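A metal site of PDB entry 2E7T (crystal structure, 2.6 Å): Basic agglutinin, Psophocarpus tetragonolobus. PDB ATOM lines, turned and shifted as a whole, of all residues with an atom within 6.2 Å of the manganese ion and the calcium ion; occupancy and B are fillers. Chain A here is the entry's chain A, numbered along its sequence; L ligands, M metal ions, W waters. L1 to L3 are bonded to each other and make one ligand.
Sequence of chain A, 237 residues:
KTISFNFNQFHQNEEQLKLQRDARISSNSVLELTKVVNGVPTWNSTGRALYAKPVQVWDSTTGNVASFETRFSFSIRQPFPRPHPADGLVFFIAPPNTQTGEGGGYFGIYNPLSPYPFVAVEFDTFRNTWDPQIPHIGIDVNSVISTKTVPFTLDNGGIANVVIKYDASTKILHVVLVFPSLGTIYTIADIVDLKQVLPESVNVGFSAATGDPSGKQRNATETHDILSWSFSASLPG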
ATOM      1  N   ASP A  87     -19.790 -30.720 -23.456  1.00  0.00           N
ATOM      2  CA  ASP A  87     -20.510 -29.901 -24.421  1.00  0.00           C
ATOM      3  C   ASP A  87     -20.513 -30.541 -25.800  1.00  0.00           C
ATOM      4  O   ASP A  87     -21.454 -30.342 -26.585  1.00  0.00           O
ATOM      5  CB  ASP A  87     -19.890 -28.500 -24.527  1.00  0.00           C
ATOM      6  CG  ASP A  87     -20.438 -27.534 -23.478  1.00  0.00           C
ATOM      7  OD1 ASP A  87     -19.858 -27.439 -22.360  1.00  0.00           O
ATOM      8  OD2 ASP A  87     -21.459 -26.859 -23.768  1.00  0.00           O
ATOM      9  N   GLY A 104     -16.551 -24.605 -23.047  1.00  0.00           N
ATOM     10  CA  GLY A 104     -17.991 -24.663 -23.081  1.00  0.00           C
ATOM     11  C   GLY A 104     -18.563 -24.861 -24.474  1.00  0.00           C
ATOM     12  O   GLY A 104     -18.071 -25.695 -25.238  1.00  0.00           O
ATOM     13  N   GLY A 105     -19.601 -24.101 -24.797  1.00  0.00           N
ATOM     14  CA  GLY A 105     -20.250 -24.211 -26.093  1.00  0.00           C
ATOM     15  C   GLY A 105     -19.399 -23.731 -27.244  1.00  0.00           C
ATOM     16  O   GLY A 105     -19.850 -23.782 -28.400  1.00  0.00           O
ATOM     17  N   PHE A 107     -16.475 -25.083 -27.791  1.00  0.00           N
ATOM     18  CA  PHE A 107     -15.668 -26.280 -28.082  1.00  0.00           C
ATOM     19  C   PHE A 107     -14.154 -26.104 -28.033  1.00  0.00           C
ATOM     20  O   PHE A 107     -13.427 -27.042 -28.283  1.00  0.00           O
ATOM     21  CB  PHE A 107     -16.049 -26.850 -29.454  1.00  0.00           C
ATOM     22  CG  PHE A 107     -17.530 -27.090 -29.642  1.00  0.00           C
ATOM     23  CD1 PHE A 107     -18.197 -28.040 -28.881  1.00  0.00           C
ATOM     24  CD2 PHE A 107     -18.246 -26.376 -30.594  1.00  0.00           C
ATOM     25  CE1 PHE A 107     -19.555 -28.301 -29.080  1.00  0.00           C
ATOM     26  CE2 PHE A 107     -19.597 -26.625 -30.796  1.00  0.00           C
ATOM     27  CZ  PHE A 107     -20.260 -27.595 -30.042  1.00  0.00           C
ATOM     28  N   GLU A 122     -19.393 -30.284 -35.962  1.00  0.00           N
ATOM     29  CA  GLU A 122     -19.630 -30.499 -34.557  1.00  0.00           C
ATOM     30  C   GLU A 122     -20.607 -31.620 -34.211  1.00  0.00           C
ATOM     31  O   GLU A 122     -21.515 -31.951 -34.973  1.00  0.00           O
ATOM     32  CB  GLU A 122     -20.131 -29.219 -33.921  1.00  0.00           C
ATOM     33  CG  GLU A 122     -21.495 -28.813 -34.442  1.00  0.00           C
ATOM     34  CD  GLU A 122     -22.143 -27.688 -33.642  1.00  0.00           C
ATOM     35  OE1 GLU A 122     -21.551 -26.594 -33.562  1.00  0.00           O
ATOM     36  OE2 GLU A 122     -23.260 -27.910 -33.101  1.00  0.00           O
ATOM     37  N   ASP A 124     -22.595 -31.768 -31.184  1.00  0.00           N
ATOM     38  CA  ASP A 124     -23.058 -30.968 -30.076  1.00  0.00           C
ATOM     39  C   ASP A 124     -23.983 -31.694 -29.157  1.00  0.00           C
ATOM     40  O   ASP A 124     -25.012 -32.206 -29.611  1.00  0.00           O
ATOM     41  CB  ASP A 124     -23.758 -29.740 -30.646  1.00  0.00           C
ATOM     42  CG  ASP A 124     -23.773 -28.577 -29.681  1.00  0.00           C
ATOM     43  OD1 ASP A 124     -23.765 -28.817 -28.457  1.00  0.00           O
ATOM     44  OD2 ASP A 124     -23.779 -27.431 -30.146  1.00  0.00           O
ATOM     45  N   THR A 125     -23.673 -31.684 -27.865  1.00  0.00           N
ATOM     46  CA  THR A 125     -24.505 -32.393 -26.893  1.00  0.00           C
ATOM     47  C   THR A 125     -25.243 -31.524 -25.868  1.00  0.00           C
ATOM     48  O   THR A 125     -26.104 -32.021 -25.141  1.00  0.00           O
ATOM     49  CB  THR A 125     -23.659 -33.430 -26.163  1.00  0.00           C
ATOM     50  OG1 THR A 125     -22.557 -32.787 -25.523  1.00  0.00           O
ATOM     51  CG2 THR A 125     -23.111 -34.461 -27.168  1.00  0.00           C
ATOM     52  N   PHE A 126     -24.906 -30.233 -25.796  1.00  0.00           N
ATOM     53  CA  PHE A 126     -25.516 -29.314 -24.858  1.00  0.00           C
ATOM     54  C   PHE A 126     -26.199 -28.234 -25.658  1.00  0.00           C
ATOM     55  O   PHE A 126     -25.642 -27.745 -26.641  1.00  0.00           O
ATOM     56  CB  PHE A 126     -24.461 -28.666 -23.964  1.00  0.00           C
ATOM     57  CG  PHE A 126     -25.020 -27.605 -23.077  1.00  0.00           C
ATOM     58  CD1 PHE A 126     -25.671 -27.934 -21.894  1.00  0.00           C
ATOM     59  CD2 PHE A 126     -24.903 -26.257 -23.431  1.00  0.00           C
ATOM     60  CE1 PHE A 126     -26.196 -26.943 -21.061  1.00  0.00           C
ATOM     61  CE2 PHE A 126     -25.419 -25.258 -22.613  1.00  0.00           C
ATOM     62  CZ  PHE A 126     -26.075 -25.591 -21.422  1.00  0.00           C
ATOM     63  N   ARG A 127     -27.410 -27.850 -25.255  1.00  0.00           N
ATOM     64  CA  ARG A 127     -28.140 -26.821 -25.994  1.00  0.00           C
ATOM     65  C   ARG A 127     -27.938 -25.395 -25.517  1.00  0.00           C
ATOM     66  O   ARG A 127     -28.514 -25.013 -24.508  1.00  0.00           O
ATOM     67  CB  ARG A 127     -29.637 -27.131 -26.010  1.00  0.00           C
ATOM     68  CG  ARG A 127     -30.424 -26.103 -26.785  1.00  0.00           C
ATOM     69  CD  ARG A 127     -31.877 -26.519 -26.954  1.00  0.00           C
ATOM     70  NE  ARG A 127     -32.528 -25.701 -27.980  1.00  0.00           N
ATOM     71  CZ  ARG A 127     -33.753 -25.919 -28.446  1.00  0.00           C
ATOM     72  NH1 ARG A 127     -34.461 -26.940 -27.974  1.00  0.00           N
ATOM     73  NH2 ARG A 127     -34.246 -25.157 -29.402  1.00  0.00           N
ATOM     74  N   ASN A 128     -27.147 -24.621 -26.238  1.00  0.00           N
ATOM     75  CA  ASN A 128     -26.941 -23.230 -25.878  1.00  0.00           C
ATOM     76  C   ASN A 128     -28.072 -22.396 -26.451  1.00  0.00           C
ATOM     77  O   ASN A 128     -28.927 -22.919 -27.161  1.00  0.00           O
ATOM     78  CB  ASN A 128     -25.603 -22.710 -26.416  1.00  0.00           C
ATOM     79  CG  ASN A 128     -24.426 -23.412 -25.800  1.00  0.00           C
ATOM     80  OD1 ASN A 128     -24.092 -24.523 -26.187  1.00  0.00           O
ATOM     81  ND2 ASN A 128     -23.803 -22.781 -24.836  1.00  0.00           N
ATOM     82  N   TRP A 130     -28.115 -20.444 -28.807  1.00  0.00           N
ATOM     83  CA  TRP A 130     -28.072 -20.462 -30.269  1.00  0.00           C
ATOM     84  C   TRP A 130     -28.289 -21.818 -30.925  1.00  0.00           C
ATOM     85  O   TRP A 130     -28.225 -21.921 -32.149  1.00  0.00           O
ATOM     86  CB  TRP A 130     -26.734 -19.900 -30.722  1.00  0.00           C
ATOM     87  CG  TRP A 130     -25.576 -20.735 -30.287  1.00  0.00           C
ATOM     88  CD1 TRP A 130     -25.177 -21.944 -30.810  1.00  0.00           C
ATOM     89  CD2 TRP A 130     -24.665 -20.447 -29.213  1.00  0.00           C
ATOM     90  NE1 TRP A 130     -24.080 -22.415 -30.128  1.00  0.00           N
ATOM     91  CE2 TRP A 130     -23.749 -21.522 -29.148  1.00  0.00           C
ATOM     92  CE3 TRP A 130     -24.528 -19.379 -28.304  1.00  0.00           C
ATOM     93  CZ2 TRP A 130     -22.704 -21.560 -28.218  1.00  0.00           C
ATOM     94  CZ3 TRP A 130     -23.490 -19.429 -27.372  1.00  0.00           C
ATOM     95  CH2 TRP A 130     -22.598 -20.505 -27.335  1.00  0.00           C
ATOM     96  N   ASP A 131     -28.575 -22.838 -30.117  1.00  0.00           N
ATOM     97  CA  ASP A 131     -28.774 -24.206 -30.590  1.00  0.00           C
ATOM     98  C   ASP A 131     -30.168 -24.748 -30.735  1.00  0.00           C
ATOM     99  O   ASP A 131     -31.083 -24.343 -30.037  1.00  0.00           O
ATOM    100  CB  ASP A 131     -28.115 -25.218 -29.643  1.00  0.00           C
ATOM    101  CG  ASP A 131     -26.628 -25.270 -29.775  1.00  0.00           C
ATOM    102  OD1 ASP A 131     -26.113 -25.120 -30.914  1.00  0.00           O
ATOM    103  OD2 ASP A 131     -25.995 -25.504 -28.712  1.00  0.00           O
ATOM    104  N   PRO A 132     -30.342 -25.722 -31.645  1.00  0.00           N
ATOM    105  CA  PRO A 132     -31.621 -26.375 -31.864  1.00  0.00           C
ATOM    106  C   PRO A 132     -31.522 -27.577 -30.910  1.00  0.00           C
ATOM    107  O   PRO A 132     -30.510 -27.726 -30.248  1.00  0.00           O
ATOM    108  CB  PRO A 132     -31.556 -26.777 -33.338  1.00  0.00           C
ATOM    109  CG  PRO A 132     -30.146 -27.100 -33.512  1.00  0.00           C
ATOM    110  CD  PRO A 132     -29.446 -25.956 -32.792  1.00  0.00           C
ATOM    111  N   ILE A 134     -30.688 -30.926 -29.019  1.00  0.00           N
ATOM    112  CA  ILE A 134     -29.466 -31.731 -29.051  1.00  0.00           C
ATOM    113  C   ILE A 134     -29.778 -33.202 -28.739  1.00  0.00           C
ATOM    114  O   ILE A 134     -30.819 -33.530 -28.191  1.00  0.00           O
ATOM    115  CB  ILE A 134     -28.392 -31.203 -28.052  1.00  0.00           C
ATOM    116  CG1 ILE A 134     -28.962 -30.989 -26.650  1.00  0.00           C
ATOM    117  CG2 ILE A 134     -27.835 -29.905 -28.580  1.00  0.00           C
ATOM    118  CD1 ILE A 134     -29.172 -32.262 -25.832  1.00  0.00           C
ATOM    119  N   HIS A 136     -26.915 -32.958 -31.946  1.00  0.00           N
ATOM    120  CA  HIS A 136     -27.058 -32.717 -33.367  1.00  0.00           C
ATOM    121  C   HIS A 136     -25.694 -32.592 -34.035  1.00  0.00           C
ATOM    122  O   HIS A 136     -24.689 -32.321 -33.384  1.00  0.00           O
ATOM    123  CB  HIS A 136     -27.893 -31.455 -33.660  1.00  0.00           C
ATOM    124  CG  HIS A 136     -27.376 -30.194 -33.019  1.00  0.00           C
ATOM    125  ND1 HIS A 136     -27.881 -29.715 -31.829  1.00  0.00           N
ATOM    126  CD2 HIS A 136     -26.446 -29.299 -33.430  1.00  0.00           C
ATOM    127  CE1 HIS A 136     -27.275 -28.567 -31.535  1.00  0.00           C
ATOM    128  NE2 HIS A 136     -26.410 -28.291 -32.485  1.00  0.00           N
ATOM    129  N   GLY A 138     -23.541 -30.573 -36.794  1.00  0.00           N
ATOM    130  CA  GLY A 138     -23.661 -29.233 -37.334  1.00  0.00           C
ATOM    131  C   GLY A 138     -22.432 -28.890 -38.143  1.00  0.00           C
ATOM    132  O   GLY A 138     -21.326 -29.394 -37.866  1.00  0.00           O
ATOM    133  N   ASP A 140     -20.083 -25.842 -39.121  1.00  0.00           N
ATOM    134  CA  ASP A 140     -19.746 -24.507 -38.682  1.00  0.00           C
ATOM    135  C   ASP A 140     -18.694 -23.830 -39.534  1.00  0.00           C
ATOM    136  O   ASP A 140     -17.676 -24.436 -39.861  1.00  0.00           O
ATOM    137  CB  ASP A 140     -19.262 -24.545 -37.230  1.00  0.00           C
ATOM    138  CG  ASP A 140     -20.273 -25.196 -36.301  1.00  0.00           C
ATOM    139  OD1 ASP A 140     -21.487 -25.236 -36.634  1.00  0.00           O
ATOM    140  OD2 ASP A 140     -19.852 -25.661 -35.216  1.00  0.00           O
ATOM    141  N   VAL A 144     -19.929 -20.980 -34.168  1.00  0.00           N
ATOM    142  CA  VAL A 144     -20.594 -22.172 -33.654  1.00  0.00           C
ATOM    143  C   VAL A 144     -22.072 -22.104 -33.928  1.00  0.00           C
ATOM    144  O   VAL A 144     -22.831 -22.920 -33.437  1.00  0.00           O
ATOM    145  CB  VAL A 144     -20.373 -22.359 -32.157  1.00  0.00           C
ATOM    146  CG1 VAL A 144     -18.878 -22.595 -31.891  1.00  0.00           C
ATOM    147  CG2 VAL A 144     -20.855 -21.133 -31.422  1.00  0.00           C
ATOM    148  N   SER A 146     -24.146 -22.964 -36.409  1.00  0.00           N
ATOM    149  CA  SER A 146     -24.157 -23.802 -37.611  1.00  0.00           C
ATOM    150  C   SER A 146     -24.984 -23.292 -38.771  1.00  0.00           C
ATOM    151  O   SER A 146     -26.045 -22.693 -38.589  1.00  0.00           O
ATOM    152  CB  SER A 146     -24.665 -25.201 -37.244  1.00  0.00           C
ATOM    153  OG  SER A 146     -23.966 -25.699 -36.131  1.00  0.00           O
ATOM    154  N   THR A 149     -27.845 -28.153 -39.725  1.00  0.00           N
ATOM    155  CA  THR A 149     -27.878 -29.015 -38.555  1.00  0.00           C
ATOM    156  C   THR A 149     -28.819 -30.208 -38.733  1.00  0.00           C
ATOM    157  O   THR A 149     -29.822 -30.121 -39.434  1.00  0.00           O
ATOM    158  CB  THR A 149     -28.336 -28.184 -37.326  1.00  0.00           C
ATOM    159  OG1 THR A 149     -27.267 -27.341 -36.874  1.00  0.00           O
ATOM    160  CG2 THR A 149     -28.771 -29.087 -36.194  1.00  0.00           C
HETATM  161  C1  LIG L   1     -27.480 -16.634 -14.559  1.00  0.00           C
HETATM  162  C2  LIG L   1     -26.578 -17.547 -13.758  1.00  0.00           C
HETATM  163  C3  LIG L   1     -25.596 -18.247 -14.663  1.00  0.00           C
HETATM  164  C4  LIG L   1     -26.276 -18.947 -15.838  1.00  0.00           C
HETATM  165  C5  LIG L   1     -27.284 -17.978 -16.536  1.00  0.00           C
HETATM  166  C6  LIG L   1     -28.179 -18.642 -17.595  1.00  0.00           C
HETATM  167  O1  LIG L   1     -26.720 -15.673 -15.181  1.00  0.00           O
HETATM  168  O2  LIG L   1     -25.864 -16.795 -12.791  1.00  0.00           O
HETATM  169  O3  LIG L   1     -24.902 -19.209 -13.900  1.00  0.00           O
HETATM  170  O4  LIG L   1     -25.247 -19.401 -16.746  1.00  0.00           O
HETATM  171  O5  LIG L   1     -28.170 -17.391 -15.564  1.00  0.00           O
HETATM  172  O6  LIG L   1     -29.262 -17.805 -17.984  1.00  0.00           O
HETATM  173  C1  LG2 L   2     -25.636 -20.089 -17.875  1.00  0.00           C
HETATM  174  C2  LG2 L   2     -24.482 -20.877 -18.477  1.00  0.00           C
HETATM  175  C3  LG2 L   2     -25.021 -21.606 -19.694  1.00  0.00           C
HETATM  176  C4  LG2 L   2     -26.219 -22.436 -19.326  1.00  0.00           C
HETATM  177  C5  LG2 L   2     -27.284 -21.586 -18.665  1.00  0.00           C
HETATM  178  C6  LG2 L   2     -28.460 -22.406 -18.189  1.00  0.00           C
HETATM  179  O1  LG2 L   2     -23.450 -19.981 -18.850  1.00  0.00           O
HETATM  180  O2  LG2 L   2     -24.064 -22.452 -20.343  1.00  0.00           O
HETATM  181  O3  LG2 L   2     -25.806 -23.436 -18.423  1.00  0.00           O
HETATM  182  O4  LG2 L   2     -26.696 -20.956 -17.518  1.00  0.00           O
HETATM  183  O5  LG2 L   2     -29.019 -21.873 -17.005  1.00  0.00           O
HETATM  184  O1  LG3 L   3     -22.597 -23.716 -19.065  1.00  0.00           O
HETATM  185  C1  LG3 L   3     -22.737 -22.594 -19.918  1.00  0.00           C
HETATM  186  C2  LG3 L   3     -21.863 -22.790 -21.174  1.00  0.00           C
HETATM  187  N1  LG3 L   3     -22.007 -21.656 -22.062  1.00  0.00           N
HETATM  188  C3  LG3 L   3     -22.289 -24.081 -21.875  1.00  0.00           C
HETATM  189  O2  LG3 L   3     -21.526 -24.348 -23.018  1.00  0.00           O
HETATM  190  C4  LG3 L   3     -22.195 -25.238 -20.914  1.00  0.00           C
HETATM  191  O3  LG3 L   3     -20.848 -25.460 -20.580  1.00  0.00           O
HETATM  192  C5  LG3 L   3     -22.984 -24.981 -19.652  1.00  0.00           C
HETATM  193  C6  LG3 L   3     -22.668 -26.043 -18.635  1.00  0.00           C
HETATM  194  O4  LG3 L   3     -23.728 -26.229 -17.735  1.00  0.00           O
HETATM  195  C7  LG3 L   3     -20.956 -21.121 -22.654  1.00  0.00           C
HETATM  196  O5  LG3 L   3     -19.833 -21.488 -22.466  1.00  0.00           O
HETATM  197  C8  LG3 L   3     -21.237 -20.008 -23.611  1.00  0.00           C
HETATM  198 MN    MN M   1     -24.619 -26.479 -32.050  1.00  0.00          MN
HETATM  199 CA    CA M   2     -23.688 -26.381 -27.719  1.00  0.00          CA
HETATM  200  O   HOH W   1     -25.557 -25.429 -33.940  1.00  0.00           O
HETATM  201  O   HOH W   2     -22.224 -24.716 -29.318  1.00  0.00           O
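OE1 of Glu 122 lies close to OD2 of Asp 140 (2.5 Å). The side-chain carboxylate of Asp 131 sits close to the indole nitrogen of Trp 130, at 3.5 Å. N of Glu 122 sits at hydrogen-bond distance from O of Gly 138 (2.9 Å). The backbone carbonyl oxygen (O) of Asp 131 sits at hydrogen-bond distance from the guanidinium group (NE) of Arg 127 (2.9 Å).
Water W2 bridges the backbone carbonyl oxygen (O) of Gly 105 and the indole nitrogen (NE1) of Trp 130.
The manganese ion is bound by OE2 of Glu 122 (2.2 Å), OD2 of Asp 124 (2.3 Å), OD1 of Asp 131 (2.3 Å), water W1 (2.4 Å) and NE2 of His 136 (2.6 Å).
OD2 of Asp 87 lies within hydrogen-bond range of O2 of LG3 L3 (2.6 Å). O2 of LG3 L3 sits at hydrogen-bond distance from ND2 of Asn 128 (3.3 Å). The backbone NH of Gly 105 is in hydrogen-bond range of an oxygen (O2) of LG3 L3 (2.6 Å).
The calcium ion is bound by the side-chain amide oxygen (OD1) of Asn 128, the side-chain carboxylate (OD1) of Asp 124, the backbone carbonyl oxygen (O) of Phe 126, the side-chain carboxylate (OD2) of Asp 124, the side-chain carboxylate (OD2) of Asp 131 and water W2. The calcium ion has six donor atoms within binding distance.
Of the 20 residues printed, 4 come within 4 Å of the calcium ion. The nearest printed residue that does not touch the calcium ion is Phe 107 (4.3 Å).
Of the 20 residues printed, 4 come within 4 Å of the manganese ion. Along chain A the residues within 4 Å of the manganese ion span positions 122 to 136.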
